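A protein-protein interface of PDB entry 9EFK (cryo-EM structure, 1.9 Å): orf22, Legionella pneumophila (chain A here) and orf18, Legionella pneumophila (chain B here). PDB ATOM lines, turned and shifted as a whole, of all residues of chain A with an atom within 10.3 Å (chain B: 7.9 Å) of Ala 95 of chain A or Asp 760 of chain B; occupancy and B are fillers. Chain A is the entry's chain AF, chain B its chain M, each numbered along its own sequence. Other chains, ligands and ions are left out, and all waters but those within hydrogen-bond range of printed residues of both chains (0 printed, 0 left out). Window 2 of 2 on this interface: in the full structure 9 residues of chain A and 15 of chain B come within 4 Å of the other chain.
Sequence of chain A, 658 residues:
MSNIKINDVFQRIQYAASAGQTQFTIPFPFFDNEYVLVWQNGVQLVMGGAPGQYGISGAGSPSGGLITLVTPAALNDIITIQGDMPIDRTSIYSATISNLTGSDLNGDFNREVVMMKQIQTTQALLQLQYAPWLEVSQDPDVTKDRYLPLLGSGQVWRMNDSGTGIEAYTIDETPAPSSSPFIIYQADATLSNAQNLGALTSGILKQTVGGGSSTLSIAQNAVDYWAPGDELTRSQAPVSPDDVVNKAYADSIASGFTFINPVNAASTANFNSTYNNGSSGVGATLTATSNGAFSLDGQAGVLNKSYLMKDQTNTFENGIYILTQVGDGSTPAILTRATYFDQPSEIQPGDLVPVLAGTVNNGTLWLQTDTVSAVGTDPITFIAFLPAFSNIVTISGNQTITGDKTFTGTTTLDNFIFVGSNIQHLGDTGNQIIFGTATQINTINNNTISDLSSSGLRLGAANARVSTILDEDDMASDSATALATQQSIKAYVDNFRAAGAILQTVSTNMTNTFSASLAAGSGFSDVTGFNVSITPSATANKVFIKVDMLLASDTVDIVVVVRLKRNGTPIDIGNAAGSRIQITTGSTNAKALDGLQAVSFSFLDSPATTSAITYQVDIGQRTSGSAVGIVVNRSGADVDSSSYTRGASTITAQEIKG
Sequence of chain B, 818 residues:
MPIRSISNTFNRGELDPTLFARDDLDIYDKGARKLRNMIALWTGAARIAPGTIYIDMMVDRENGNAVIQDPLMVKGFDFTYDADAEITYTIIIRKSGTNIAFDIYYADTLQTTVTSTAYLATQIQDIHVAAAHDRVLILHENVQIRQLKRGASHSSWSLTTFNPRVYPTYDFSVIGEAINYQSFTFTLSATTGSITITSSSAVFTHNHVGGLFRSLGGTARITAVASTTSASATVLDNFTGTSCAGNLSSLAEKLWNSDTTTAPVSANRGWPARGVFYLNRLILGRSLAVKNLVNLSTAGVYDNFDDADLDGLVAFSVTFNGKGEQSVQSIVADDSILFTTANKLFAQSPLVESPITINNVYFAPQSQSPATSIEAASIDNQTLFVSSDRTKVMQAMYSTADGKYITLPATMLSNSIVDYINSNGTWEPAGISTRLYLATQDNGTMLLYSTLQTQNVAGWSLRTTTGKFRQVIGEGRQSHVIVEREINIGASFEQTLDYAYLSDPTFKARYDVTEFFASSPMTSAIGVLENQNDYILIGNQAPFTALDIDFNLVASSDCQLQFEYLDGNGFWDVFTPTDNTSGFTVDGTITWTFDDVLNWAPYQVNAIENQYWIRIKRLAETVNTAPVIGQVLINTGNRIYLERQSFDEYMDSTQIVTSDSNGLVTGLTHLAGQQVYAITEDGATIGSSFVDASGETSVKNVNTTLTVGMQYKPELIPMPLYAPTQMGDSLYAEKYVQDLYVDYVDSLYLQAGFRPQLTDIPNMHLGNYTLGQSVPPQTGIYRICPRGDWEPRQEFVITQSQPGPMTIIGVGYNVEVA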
ATOM      1  N   ARG A  89      -6.121  24.672 -23.099  1.00  0.00           N
ATOM      2  CA  ARG A  89      -4.710  24.335 -22.923  1.00  0.00           C
ATOM      3  C   ARG A  89      -4.604  23.460 -21.679  1.00  0.00           C
ATOM      4  O   ARG A  89      -4.637  23.968 -20.558  1.00  0.00           O
ATOM      5  CB  ARG A  89      -3.849  25.584 -22.805  1.00  0.00           C
ATOM      6  CG  ARG A  89      -2.369  25.291 -22.754  1.00  0.00           C
ATOM      7  CD  ARG A  89      -1.542  26.527 -23.019  1.00  0.00           C
ATOM      8  NE  ARG A  89      -0.117  26.225 -23.022  1.00  0.00           N
ATOM      9  CZ  ARG A  89       0.667  26.298 -21.958  1.00  0.00           C
ATOM     10  NH1 ARG A  89       0.205  26.689 -20.785  1.00  0.00           N
ATOM     11  NH2 ARG A  89       1.949  25.971 -22.075  1.00  0.00           N
ATOM     12  N   ILE A  92       0.662  21.901 -19.620  1.00  0.00           N
ATOM     13  CA  ILE A  92       1.394  23.099 -19.249  1.00  0.00           C
ATOM     14  C   ILE A  92       2.793  22.700 -18.809  1.00  0.00           C
ATOM     15  O   ILE A  92       3.065  21.544 -18.484  1.00  0.00           O
ATOM     16  CB  ILE A  92       0.680  23.891 -18.140  1.00  0.00           C
ATOM     17  CG1 ILE A  92       0.654  23.076 -16.848  1.00  0.00           C
ATOM     18  CG2 ILE A  92      -0.725  24.253 -18.572  1.00  0.00           C
ATOM     19  CD1 ILE A  92       0.003  23.785 -15.697  1.00  0.00           C
ATOM     20  N   TYR A  93       3.689  23.680 -18.811  1.00  0.00           N
ATOM     21  CA  TYR A  93       5.060  23.448 -18.396  1.00  0.00           C
ATOM     22  C   TYR A  93       5.178  23.508 -16.878  1.00  0.00           C
ATOM     23  O   TYR A  93       4.304  24.022 -16.179  1.00  0.00           O
ATOM     24  CB  TYR A  93       5.993  24.478 -19.024  1.00  0.00           C
ATOM     25  CG  TYR A  93       5.907  24.554 -20.527  1.00  0.00           C
ATOM     26  CD1 TYR A  93       6.404  23.534 -21.319  1.00  0.00           C
ATOM     27  CD2 TYR A  93       5.334  25.648 -21.152  1.00  0.00           C
ATOM     28  CE1 TYR A  93       6.324  23.599 -22.689  1.00  0.00           C
ATOM     29  CE2 TYR A  93       5.254  25.720 -22.522  1.00  0.00           C
ATOM     30  CZ  TYR A  93       5.753  24.696 -23.285  1.00  0.00           C
ATOM     31  OH  TYR A  93       5.677  24.764 -24.652  1.00  0.00           O
ATOM     32  N   SER A  94       6.282  22.970 -16.370  1.00  0.00           N
ATOM     33  CA  SER A  94       6.592  23.126 -14.961  1.00  0.00           C
ATOM     34  C   SER A  94       7.019  24.562 -14.677  1.00  0.00           C
ATOM     35  O   SER A  94       7.321  25.334 -15.586  1.00  0.00           O
ATOM     36  CB  SER A  94       7.691  22.154 -14.544  1.00  0.00           C
ATOM     37  OG  SER A  94       7.306  20.823 -14.812  1.00  0.00           O
ATOM     38  N   ALA A  95       7.034  24.918 -13.392  1.00  0.00           N
ATOM     39  CA  ALA A  95       7.371  26.285 -13.012  1.00  0.00           C
ATOM     40  C   ALA A  95       8.784  26.649 -13.450  1.00  0.00           C
ATOM     41  O   ALA A  95       9.012  27.726 -14.009  1.00  0.00           O
ATOM     42  CB  ALA A  95       7.210  26.468 -11.505  1.00  0.00           C
ATOM     43  N   THR A  96       9.748  25.760 -13.216  1.00  0.00           N
ATOM     44  CA  THR A  96      11.136  25.974 -13.630  1.00  0.00           C
ATOM     45  C   THR A  96      11.570  24.769 -14.458  1.00  0.00           C
ATOM     46  O   THR A  96      12.165  23.824 -13.944  1.00  0.00           O
ATOM     47  CB  THR A  96      12.056  26.195 -12.430  1.00  0.00           C
ATOM     48  OG1 THR A  96      11.782  25.213 -11.426  1.00  0.00           O
ATOM     49  CG2 THR A  96      11.854  27.577 -11.851  1.00  0.00           C
ATOM     50  N   ILE A  97      11.281  24.817 -15.754  1.00  0.00           N
ATOM     51  CA  ILE A  97      11.667  23.730 -16.642  1.00  0.00           C
ATOM     52  C   ILE A  97      13.172  23.755 -16.860  1.00  0.00           C
ATOM     53  O   ILE A  97      13.791  24.822 -16.937  1.00  0.00           O
ATOM     54  CB  ILE A  97      10.918  23.840 -17.979  1.00  0.00           C
ATOM     55  CG1 ILE A  97      11.046  25.256 -18.535  1.00  0.00           C
ATOM     56  CG2 ILE A  97       9.471  23.463 -17.805  1.00  0.00           C
ATOM     57  CD1 ILE A  97      10.440  25.427 -19.898  1.00  0.00           C
ATOM     58  N   SER A  98      13.771  22.570 -16.952  1.00  0.00           N
ATOM     59  CA  SER A  98      15.164  22.438 -17.350  1.00  0.00           C
ATOM     60  C   SER A  98      15.308  21.677 -18.658  1.00  0.00           C
ATOM     61  O   SER A  98      16.425  21.311 -19.032  1.00  0.00           O
ATOM     62  CB  SER A  98      15.981  21.750 -16.256  1.00  0.00           C
ATOM     63  OG  SER A  98      15.723  20.364 -16.239  1.00  0.00           O
ATOM     64  N   ASN A  99      14.208  21.418 -19.355  1.00  0.00           N
ATOM     65  CA  ASN A  99      14.255  20.755 -20.653  1.00  0.00           C
ATOM     66  C   ASN A  99      13.000  21.159 -21.410  1.00  0.00           C
ATOM     67  O   ASN A  99      11.894  20.769 -21.032  1.00  0.00           O
ATOM     68  CB  ASN A  99      14.351  19.241 -20.503  1.00  0.00           C
ATOM     69  CG  ASN A  99      14.648  18.544 -21.813  1.00  0.00           C
ATOM     70  OD1 ASN A  99      13.969  18.755 -22.810  1.00  0.00           O
ATOM     71  ND2 ASN A  99      15.679  17.718 -21.818  1.00  0.00           N
ATOM     72  N   TYR B 749      15.360  23.513  -9.877  1.00  0.00           N
ATOM     73  CA  TYR B 749      13.964  23.607  -9.446  1.00  0.00           C
ATOM     74  C   TYR B 749      13.815  24.232  -8.061  1.00  0.00           C
ATOM     75  O   TYR B 749      12.949  23.840  -7.282  1.00  0.00           O
ATOM     76  CB  TYR B 749      13.291  22.235  -9.476  1.00  0.00           C
ATOM     77  CG  TYR B 749      13.629  21.412 -10.689  1.00  0.00           C
ATOM     78  CD1 TYR B 749      13.493  21.933 -11.964  1.00  0.00           C
ATOM     79  CD2 TYR B 749      14.111  20.123 -10.557  1.00  0.00           C
ATOM     80  CE1 TYR B 749      13.808  21.183 -13.074  1.00  0.00           C
ATOM     81  CE2 TYR B 749      14.429  19.370 -11.657  1.00  0.00           C
ATOM     82  CZ  TYR B 749      14.274  19.902 -12.911  1.00  0.00           C
ATOM     83  OH  TYR B 749      14.596  19.148 -14.007  1.00  0.00           O
ATOM     84  N   LEU B 750      14.646  25.216  -7.748  1.00  0.00           N
ATOM     85  CA  LEU B 750      14.567  25.835  -6.435  1.00  0.00           C
ATOM     86  C   LEU B 750      13.455  26.876  -6.382  1.00  0.00           C
ATOM     87  O   LEU B 750      13.032  27.426  -7.399  1.00  0.00           O
ATOM     88  CB  LEU B 750      15.896  26.485  -6.066  1.00  0.00           C
ATOM     89  CG  LEU B 750      17.112  25.566  -6.034  1.00  0.00           C
ATOM     90  CD1 LEU B 750      18.355  26.356  -5.689  1.00  0.00           C
ATOM     91  CD2 LEU B 750      16.892  24.444  -5.044  1.00  0.00           C
ATOM     92  N   GLN B 751      12.972  27.135  -5.170  1.00  0.00           N
ATOM     93  CA  GLN B 751      12.070  28.249  -4.919  1.00  0.00           C
ATOM     94  C   GLN B 751      12.234  28.694  -3.477  1.00  0.00           C
ATOM     95  O   GLN B 751      12.471  27.870  -2.593  1.00  0.00           O
ATOM     96  CB  GLN B 751      10.609  27.892  -5.212  1.00  0.00           C
ATOM     97  CG  GLN B 751      10.171  26.552  -4.695  1.00  0.00           C
ATOM     98  CD  GLN B 751       8.696  26.300  -4.926  1.00  0.00           C
ATOM     99  OE1 GLN B 751       8.044  27.013  -5.681  1.00  0.00           O
ATOM    100  NE2 GLN B 751       8.162  25.281  -4.269  1.00  0.00           N
ATOM    101  N   ALA B 752      12.118  29.997  -3.246  1.00  0.00           N
ATOM    102  CA  ALA B 752      12.433  30.561  -1.945  1.00  0.00           C
ATOM    103  C   ALA B 752      11.578  31.789  -1.693  1.00  0.00           C
ATOM    104  O   ALA B 752      11.036  32.391  -2.620  1.00  0.00           O
ATOM    105  CB  ALA B 752      13.914  30.927  -1.842  1.00  0.00           C
ATOM    106  N   GLY B 753      11.469  32.159  -0.427  1.00  0.00           N
ATOM    107  CA  GLY B 753      10.831  33.401  -0.068  1.00  0.00           C
ATOM    108  C   GLY B 753      10.011  33.259   1.193  1.00  0.00           C
ATOM    109  O   GLY B 753      10.261  32.391   2.026  1.00  0.00           O
ATOM    110  N   GLN B 757       3.488  33.371  -0.997  1.00  0.00           N
ATOM    111  CA  GLN B 757       3.901  33.691  -2.363  1.00  0.00           C
ATOM    112  C   GLN B 757       5.420  33.618  -2.446  1.00  0.00           C
ATOM    113  O   GLN B 757       6.121  34.533  -2.014  1.00  0.00           O
ATOM    114  CB  GLN B 757       3.386  35.064  -2.774  1.00  0.00           C
ATOM    115  CG  GLN B 757       3.779  35.471  -4.176  1.00  0.00           C
ATOM    116  CD  GLN B 757       3.259  34.511  -5.217  1.00  0.00           C
ATOM    117  OE1 GLN B 757       2.054  34.409  -5.435  1.00  0.00           O
ATOM    118  NE2 GLN B 757       4.164  33.794  -5.865  1.00  0.00           N
ATOM    119  N   LEU B 758       5.926  32.530  -3.013  1.00  0.00           N
ATOM    120  CA  LEU B 758       7.356  32.316  -3.160  1.00  0.00           C
ATOM    121  C   LEU B 758       7.821  32.741  -4.546  1.00  0.00           C
ATOM    122  O   LEU B 758       7.028  33.075  -5.426  1.00  0.00           O
ATOM    123  CB  LEU B 758       7.712  30.850  -2.909  1.00  0.00           C
ATOM    124  CG  LEU B 758       7.330  30.273  -1.548  1.00  0.00           C
ATOM    125  CD1 LEU B 758       7.893  28.880  -1.399  1.00  0.00           C
ATOM    126  CD2 LEU B 758       7.817  31.169  -0.428  1.00  0.00           C
ATOM    127  N   THR B 759       9.134  32.721  -4.730  1.00  0.00           N
ATOM    128  CA  THR B 759       9.761  33.066  -5.996  1.00  0.00           C
ATOM    129  C   THR B 759      10.525  31.857  -6.509  1.00  0.00           C
ATOM    130  O   THR B 759      11.335  31.278  -5.781  1.00  0.00           O
ATOM    131  CB  THR B 759      10.705  34.261  -5.836  1.00  0.00           C
ATOM    132  OG1 THR B 759       9.970  35.388  -5.347  1.00  0.00           O
ATOM    133  CG2 THR B 759      11.338  34.619  -7.161  1.00  0.00           C
ATOM    134  N   ASP B 760      10.261  31.473  -7.752  1.00  0.00           N
ATOM    135  CA  ASP B 760      11.000  30.390  -8.378  1.00  0.00           C
ATOM    136  C   ASP B 760      12.343  30.899  -8.882  1.00  0.00           C
ATOM    137  O   ASP B 760      12.440  32.005  -9.417  1.00  0.00           O
ATOM    138  CB  ASP B 760      10.200  29.792  -9.531  1.00  0.00           C
ATOM    139  CG  ASP B 760       8.910  29.150  -9.072  1.00  0.00           C
ATOM    140  OD1 ASP B 760       8.963  28.221  -8.241  1.00  0.00           O
ATOM    141  OD2 ASP B 760       7.837  29.584  -9.535  1.00  0.00           O
ATOM    142  N   ILE B 761      13.379  30.091  -8.705  1.00  0.00           N
ATOM    143  CA  ILE B 761      14.726  30.423  -9.155  1.00  0.00           C
ATOM    144  C   ILE B 761      14.934  29.788 -10.526  1.00  0.00           C
ATOM    145  O   ILE B 761      14.924  28.554 -10.627  1.00  0.00           O
ATOM    146  CB  ILE B 761      15.790  29.942  -8.160  1.00  0.00           C
ATOM    147  CG1 ILE B 761      15.605  30.644  -6.815  1.00  0.00           C
ATOM    148  CG2 ILE B 761      17.175  30.191  -8.714  1.00  0.00           C
ATOM    149  CD1 ILE B 761      16.611  30.241  -5.773  1.00  0.00           C
ATOM    150  N   PRO B 762      15.120  30.570 -11.584  1.00  0.00           N
ATOM    151  CA  PRO B 762      15.223  29.989 -12.926  1.00  0.00           C
ATOM    152  C   PRO B 762      16.481  29.152 -13.098  1.00  0.00           C
ATOM    153  O   PRO B 762      17.512  29.396 -12.469  1.00  0.00           O
ATOM    154  CB  PRO B 762      15.251  31.215 -13.844  1.00  0.00           C
ATOM    155  CG  PRO B 762      14.769  32.351 -13.003  1.00  0.00           C
ATOM    156  CD  PRO B 762      15.193  32.037 -11.616  1.00  0.00           C
ATOM    157  N   ASN B 763      16.377  28.144 -13.960  1.00  0.00           N
ATOM    158  CA  ASN B 763      17.519  27.331 -14.367  1.00  0.00           C
ATOM    159  C   ASN B 763      17.480  27.087 -15.873  1.00  0.00           C
ATOM    160  O   ASN B 763      17.571  25.955 -16.346  1.00  0.00           O
ATOM    161  CB  ASN B 763      17.581  26.011 -13.599  1.00  0.00           C
ATOM    162  CG  ASN B 763      16.224  25.367 -13.413  1.00  0.00           C
ATOM    163  OD1 ASN B 763      15.725  25.273 -12.299  1.00  0.00           O
ATOM    164  ND2 ASN B 763      15.630  24.907 -14.500  1.00  0.00           N
ATOM    165  N   TYR B 782      21.205  33.909  -6.152  1.00  0.00           N
ATOM    166  CA  TYR B 782      19.991  34.558  -6.619  1.00  0.00           C
ATOM    167  C   TYR B 782      19.461  35.476  -5.528  1.00  0.00           C
ATOM    168  O   TYR B 782      19.393  35.085  -4.361  1.00  0.00           O
ATOM    169  CB  TYR B 782      18.935  33.530  -7.021  1.00  0.00           C
ATOM    170  CG  TYR B 782      17.911  34.077  -7.980  1.00  0.00           C
ATOM    171  CD1 TYR B 782      18.240  34.336  -9.301  1.00  0.00           C
ATOM    172  CD2 TYR B 782      16.618  34.338  -7.567  1.00  0.00           C
ATOM    173  CE1 TYR B 782      17.308  34.837 -10.179  1.00  0.00           C
ATOM    174  CE2 TYR B 782      15.681  34.839  -8.436  1.00  0.00           C
ATOM    175  CZ  TYR B 782      16.031  35.088  -9.740  1.00  0.00           C
ATOM    176  OH  TYR B 782      15.094  35.587 -10.611  1.00  0.00           O
ATOM    177  N   ILE B 784      16.406  37.919  -4.028  1.00  0.00           N
ATOM    178  CA  ILE B 784      14.948  37.903  -4.004  1.00  0.00           C
ATOM    179  C   ILE B 784      14.458  38.936  -3.000  1.00  0.00           C
ATOM    180  O   ILE B 784      15.030  39.079  -1.917  1.00  0.00           O
ATOM    181  CB  ILE B 784      14.423  36.497  -3.641  1.00  0.00           C
ATOM    182  CG1 ILE B 784      14.664  35.519  -4.787  1.00  0.00           C
ATOM    183  CG2 ILE B 784      12.958  36.533  -3.275  1.00  0.00           C
ATOM    184  CD1 ILE B 784      14.391  34.090  -4.416  1.00  0.00           C
ATOM    185  N   THR B 799      13.013  25.662  -0.753  1.00  0.00           N
ATOM    186  CA  THR B 799      12.415  24.367  -1.046  1.00  0.00           C
ATOM    187  C   THR B 799      12.570  24.088  -2.537  1.00  0.00           C
ATOM    188  O   THR B 799      13.232  24.835  -3.260  1.00  0.00           O
ATOM    189  CB  THR B 799      10.958  24.340  -0.565  1.00  0.00           C
ATOM    190  OG1 THR B 799      10.425  23.016  -0.683  1.00  0.00           O
ATOM    191  CG2 THR B 799      10.100  25.297  -1.362  1.00  0.00           C
ATOM    192  N   GLN B 800      11.968  22.995  -2.996  1.00  0.00           N
ATOM    193  CA  GLN B 800      12.122  22.514  -4.361  1.00  0.00           C
ATOM    194  C   GLN B 800      10.750  22.209  -4.937  1.00  0.00           C
ATOM    195  O   GLN B 800       9.928  21.578  -4.270  1.00  0.00           O
ATOM    196  CB  GLN B 800      13.002  21.265  -4.388  1.00  0.00           C
ATOM    197  CG  GLN B 800      13.778  21.063  -5.656  1.00  0.00           C
ATOM    198  CD  GLN B 800      14.640  19.827  -5.603  1.00  0.00           C
ATOM    199  OE1 GLN B 800      14.241  18.810  -5.052  1.00  0.00           O
ATOM    200  NE2 GLN B 800      15.829  19.912  -6.172  1.00  0.00           N
ATOM    201  N   SER B 801      10.501  22.648  -6.172  1.00  0.00           N
ATOM    202  CA  SER B 801       9.191  22.428  -6.775  1.00  0.00           C
ATOM    203  C   SER B 801       9.003  20.997  -7.269  1.00  0.00           C
ATOM    204  O   SER B 801       7.889  20.471  -7.200  1.00  0.00           O
ATOM    205  CB  SER B 801       8.955  23.419  -7.916  1.00  0.00           C
ATOM    206  OG  SER B 801      10.043  23.443  -8.816  1.00  0.00           O
ATOM    207  N   GLN B 802      10.052  20.359  -7.774  1.00  0.00           N
ATOM    208  CA  GLN B 802       9.972  18.983  -8.241  1.00  0.00           C
ATOM    209  C   GLN B 802      11.311  18.313  -7.977  1.00  0.00           C
ATOM    210  O   GLN B 802      12.320  19.001  -7.790  1.00  0.00           O
ATOM    211  CB  GLN B 802       9.593  18.915  -9.726  1.00  0.00           C
ATOM    212  CG  GLN B 802      10.501  19.673 -10.660  1.00  0.00           C
ATOM    213  CD  GLN B 802      10.013  19.622 -12.090  1.00  0.00           C
ATOM    214  OE1 GLN B 802       8.935  19.105 -12.368  1.00  0.00           O
ATOM    215  NE2 GLN B 802      10.805  20.154 -13.006  1.00  0.00           N
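OH of Tyr 749 of chain B lies within hydrogen-bond range of OG of Ser 98 of chain A. OG of Ser 94 of chain A is in hydrogen-bond range of OE1 of Gln 802 of chain B. The side-chain amide nitrogen of Asn 763 of chain B sits at hydrogen-bond distance from the backbone carbonyl oxygen of Ile 97 of chain A (3.1 Å).
The side-chain amide oxygen (OE1) of Gln 800 of chain B lies close to the backbone carbonyl oxygen (O) of Gln 802 of chain B (3.4 Å). OE1 of Gln 751 of chain B lies close to OD1 of Asp 760 of chain B, 3.0 Å away. The backbone NH (N) of Ser 801 of chain B sits at hydrogen-bond distance from the backbone carbonyl oxygen (O) of Tyr 749 of chain B. O of Leu 750 of chain B lies within hydrogen-bond range of N of Ile 761 of chain B (3.0 Å). The side-chain amide oxygen of Asn 763 of chain B sits at hydrogen-bond distance from the backbone NH of Tyr 749 of chain B, 3.0 Å away.
Among the printed residues, pairs that only touch across the chains: Thr 96 of chain A with Tyr 749 of chain B, Thr 96 of chain A with Ile 761 of chain B, Thr 96 of chain A with Ser 801 of chain B, Thr 96 of chain A with Asp 760 of chain B, Ser 98 of chain A with Asn 763 of chain B, Thr 96 of chain A with Asn 763 of chain B and Ala 95 of chain A with Asp 760 of chain B.
Ala 95 of chain A touches one residue of chain B. Thr 759 of chain B touches none of the printed residues of chain A. Asp 760 of chain B touches just these residues of chain A: Ala 95 (3.7 Å) and Thr 96 (3.6 Å). Printed residues of chain A within 4 Å of Asn 763 of chain B: Thr 96 (3.7 Å), Ile 97 (3.1 Å) and Ser 98 (3.6 Å). Printed residues of chain A within 4 Å of Gln 802 of chain B: Ser 94 (3.4 Å).
Printed residues of chain B that touch a printed residue of chain A: Tyr 749, Asp 760, Ile 761, Asn 763, Ser 801 and Gln 802. Along chain B the printed residues that touch a printed residue of chain A span positions 749 to 802. Of the 9 printed residues of chain A, 5 touch a printed residue of chain B. Among the printed residues, 10 pairs touch across the chains. Among the printed residues, no Asp or Glu carboxylate lies within 4 Å of a Lys or Arg side-chain nitrogen of the other chain.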
